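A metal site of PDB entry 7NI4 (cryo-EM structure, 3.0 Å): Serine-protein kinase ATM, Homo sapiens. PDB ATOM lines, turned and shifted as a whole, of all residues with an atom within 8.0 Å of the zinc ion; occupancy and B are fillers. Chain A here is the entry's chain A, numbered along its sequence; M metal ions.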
ATOM      1  N   SER A1872      14.427  13.309   2.993  1.00  0.00           N
ATOM      2  CA  SER A1872      15.585  12.451   3.193  1.00  0.00           C
ATOM      3  C   SER A1872      16.000  11.751   1.903  1.00  0.00           C
ATOM      4  O   SER A1872      17.166  11.386   1.735  1.00  0.00           O
ATOM      5  CB  SER A1872      15.291  11.429   4.295  1.00  0.00           C
ATOM      6  OG  SER A1872      14.677  12.075   5.390  1.00  0.00           O
ATOM      7  N   ARG A1875      18.887  13.704  -0.065  1.00  0.00           N
ATOM      8  CA  ARG A1875      20.265  13.947   0.468  1.00  0.00           C
ATOM      9  C   ARG A1875      21.209  13.778  -0.713  1.00  0.00           C
ATOM     10  O   ARG A1875      20.885  12.941  -1.580  1.00  0.00           O
ATOM     11  CB  ARG A1875      20.591  12.998   1.619  1.00  0.00           C
ATOM     12  CG  ARG A1875      19.751  13.237   2.856  1.00  0.00           C
ATOM     13  CD  ARG A1875      19.664  14.717   3.205  1.00  0.00           C
ATOM     14  NE  ARG A1875      18.490  14.999   4.009  1.00  0.00           N
ATOM     15  CZ  ARG A1875      18.460  14.981   5.338  1.00  0.00           C
ATOM     16  NH1 ARG A1875      19.559  14.691   6.015  1.00  0.00           N
ATOM     17  NH2 ARG A1875      17.344  15.248   5.980  1.00  0.00           N
ATOM     18  N   HIS A1876      22.305  14.544  -0.758  1.00  0.00           N
ATOM     19  CA  HIS A1876      23.247  14.549  -1.923  1.00  0.00           C
ATOM     20  C   HIS A1876      22.643  15.407  -3.046  1.00  0.00           C
ATOM     21  O   HIS A1876      21.809  14.864  -3.781  1.00  0.00           O
ATOM     22  CB  HIS A1876      23.614  13.145  -2.411  1.00  0.00           C
ATOM     23  CG  HIS A1876      24.108  12.228  -1.339  1.00  0.00           C
ATOM     24  ND1 HIS A1876      25.412  12.244  -0.902  1.00  0.00           N
ATOM     25  CD2 HIS A1876      23.477  11.289  -0.624  1.00  0.00           C
ATOM     26  CE1 HIS A1876      25.562  11.340   0.035  1.00  0.00           C
ATOM     27  NE2 HIS A1876      24.384  10.735   0.230  1.00  0.00           N
ATOM     28  N   HIS A1895      27.863   8.960   5.467  1.00  0.00           N
ATOM     29  CA  HIS A1895      27.983  10.434   5.277  1.00  0.00           C
ATOM     30  C   HIS A1895      26.735  11.122   5.836  1.00  0.00           C
ATOM     31  O   HIS A1895      26.878  12.250   6.360  1.00  0.00           O
ATOM     32  CB  HIS A1895      28.264  10.748   3.795  1.00  0.00           C
ATOM     33  CG  HIS A1895      27.485   9.891   2.871  1.00  0.00           C
ATOM     34  ND1 HIS A1895      28.029   9.311   1.747  1.00  0.00           N
ATOM     35  CD2 HIS A1895      26.194   9.494   2.920  1.00  0.00           C
ATOM     36  CE1 HIS A1895      27.102   8.601   1.130  1.00  0.00           C
ATOM     37  NE2 HIS A1895      25.962   8.711   1.830  1.00  0.00           N
ATOM     38  N   PHE A1896      25.566  10.494   5.732  1.00  0.00           N
ATOM     39  CA  PHE A1896      24.315  11.055   6.329  1.00  0.00           C
ATOM     40  C   PHE A1896      23.598   9.960   7.117  1.00  0.00           C
ATOM     41  O   PHE A1896      23.670   8.789   6.706  1.00  0.00           O
ATOM     42  CB  PHE A1896      23.416  11.666   5.255  1.00  0.00           C
ATOM     43  CG  PHE A1896      24.016  12.815   4.485  1.00  0.00           C
ATOM     44  CD1 PHE A1896      24.200  14.050   5.080  1.00  0.00           C
ATOM     45  CD2 PHE A1896      24.381  12.662   3.157  1.00  0.00           C
ATOM     46  CE1 PHE A1896      24.750  15.102   4.378  1.00  0.00           C
ATOM     47  CE2 PHE A1896      24.938  13.719   2.451  1.00  0.00           C
ATOM     48  CZ  PHE A1896      25.115  14.936   3.058  1.00  0.00           C
ATOM     49  N   PHE A1897      22.933  10.331   8.207  1.00  0.00           N
ATOM     50  CA  PHE A1897      22.249   9.326   9.078  1.00  0.00           C
ATOM     51  C   PHE A1897      21.145   8.631   8.279  1.00  0.00           C
ATOM     52  O   PHE A1897      21.049   7.384   8.363  1.00  0.00           O
ATOM     53  CB  PHE A1897      21.662  10.020  10.308  1.00  0.00           C
ATOM     54  CG  PHE A1897      20.705   9.180  11.131  1.00  0.00           C
ATOM     55  CD1 PHE A1897      21.124   7.999  11.722  1.00  0.00           C
ATOM     56  CD2 PHE A1897      19.393   9.589  11.326  1.00  0.00           C
ATOM     57  CE1 PHE A1897      20.252   7.233  12.478  1.00  0.00           C
ATOM     58  CE2 PHE A1897      18.520   8.818  12.075  1.00  0.00           C
ATOM     59  CZ  PHE A1897      18.953   7.643  12.648  1.00  0.00           C
ATOM     60  N   ARG A1898      20.361   9.382   7.516  1.00  0.00           N
ATOM     61  CA  ARG A1898      19.307   8.773   6.656  1.00  0.00           C
ATOM     62  C   ARG A1898      19.526   9.296   5.230  1.00  0.00           C
ATOM     63  O   ARG A1898      19.333  10.503   5.008  1.00  0.00           O
ATOM     64  CB  ARG A1898      17.920   9.073   7.219  1.00  0.00           C
ATOM     65  CG  ARG A1898      17.598   8.325   8.500  1.00  0.00           C
ATOM     66  CD  ARG A1898      17.633   6.821   8.291  1.00  0.00           C
ATOM     67  NE  ARG A1898      17.791   6.083   9.539  1.00  0.00           N
ATOM     68  CZ  ARG A1898      16.785   5.622  10.266  1.00  0.00           C
ATOM     69  NH1 ARG A1898      15.538   5.824   9.886  1.00  0.00           N
ATOM     70  NH2 ARG A1898      17.026   4.966  11.382  1.00  0.00           N
ATOM     71  N   CYS A1899      19.906   8.411   4.297  1.00  0.00           N
ATOM     72  CA  CYS A1899      20.252   8.871   2.931  1.00  0.00           C
ATOM     73  C   CYS A1899      20.353   7.694   1.968  1.00  0.00           C
ATOM     74  O   CYS A1899      20.316   6.540   2.444  1.00  0.00           O
ATOM     75  CB  CYS A1899      21.602   9.553   2.940  1.00  0.00           C
ATOM     76  SG  CYS A1899      22.964   8.375   2.958  1.00  0.00           S
ATOM     77  N   CYS A1900      20.456   7.974   0.663  1.00  0.00           N
ATOM     78  CA  CYS A1900      20.672   6.905  -0.342  1.00  0.00           C
ATOM     79  C   CYS A1900      19.591   5.824  -0.219  1.00  0.00           C
ATOM     80  O   CYS A1900      19.954   4.635  -0.211  1.00  0.00           O
ATOM     81  CB  CYS A1900      22.070   6.323  -0.197  1.00  0.00           C
ATOM     82  SG  CYS A1900      23.395   7.462  -0.662  1.00  0.00           S
ATOM     83  N   LEU A1901      18.332   6.223  -0.116  1.00  0.00           N
ATOM     84  CA  LEU A1901      17.212   5.253   0.019  1.00  0.00           C
ATOM     85  C   LEU A1901      17.093   4.407  -1.252  1.00  0.00           C
ATOM     86  O   LEU A1901      17.332   4.962  -2.338  1.00  0.00           O
ATOM     87  CB  LEU A1901      15.920   6.024   0.283  1.00  0.00           C
ATOM     88  CG  LEU A1901      15.605   6.289   1.751  1.00  0.00           C
ATOM     89  CD1 LEU A1901      16.048   5.102   2.586  1.00  0.00           C
ATOM     90  CD2 LEU A1901      16.275   7.570   2.228  1.00  0.00           C
HETATM   91 ZN    ZN M   1      24.156   8.915   1.033  1.00  0.00          ZN
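Four residues have an atom within 4 Å of the zinc ion: His 1876, His 1895, Cys 1899 and Cys 1900.
The nearest printed residue that does not touch the zinc ion is Phe 1896 (4.3 Å).
The zinc ion is bound by a ring nitrogen (NE2) of His 1895, a ring nitrogen (NE2) of His 1876, the side-chain sulfur (SG) of Cys 1899 and the side-chain sulfur (SG) of Cys 1900.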
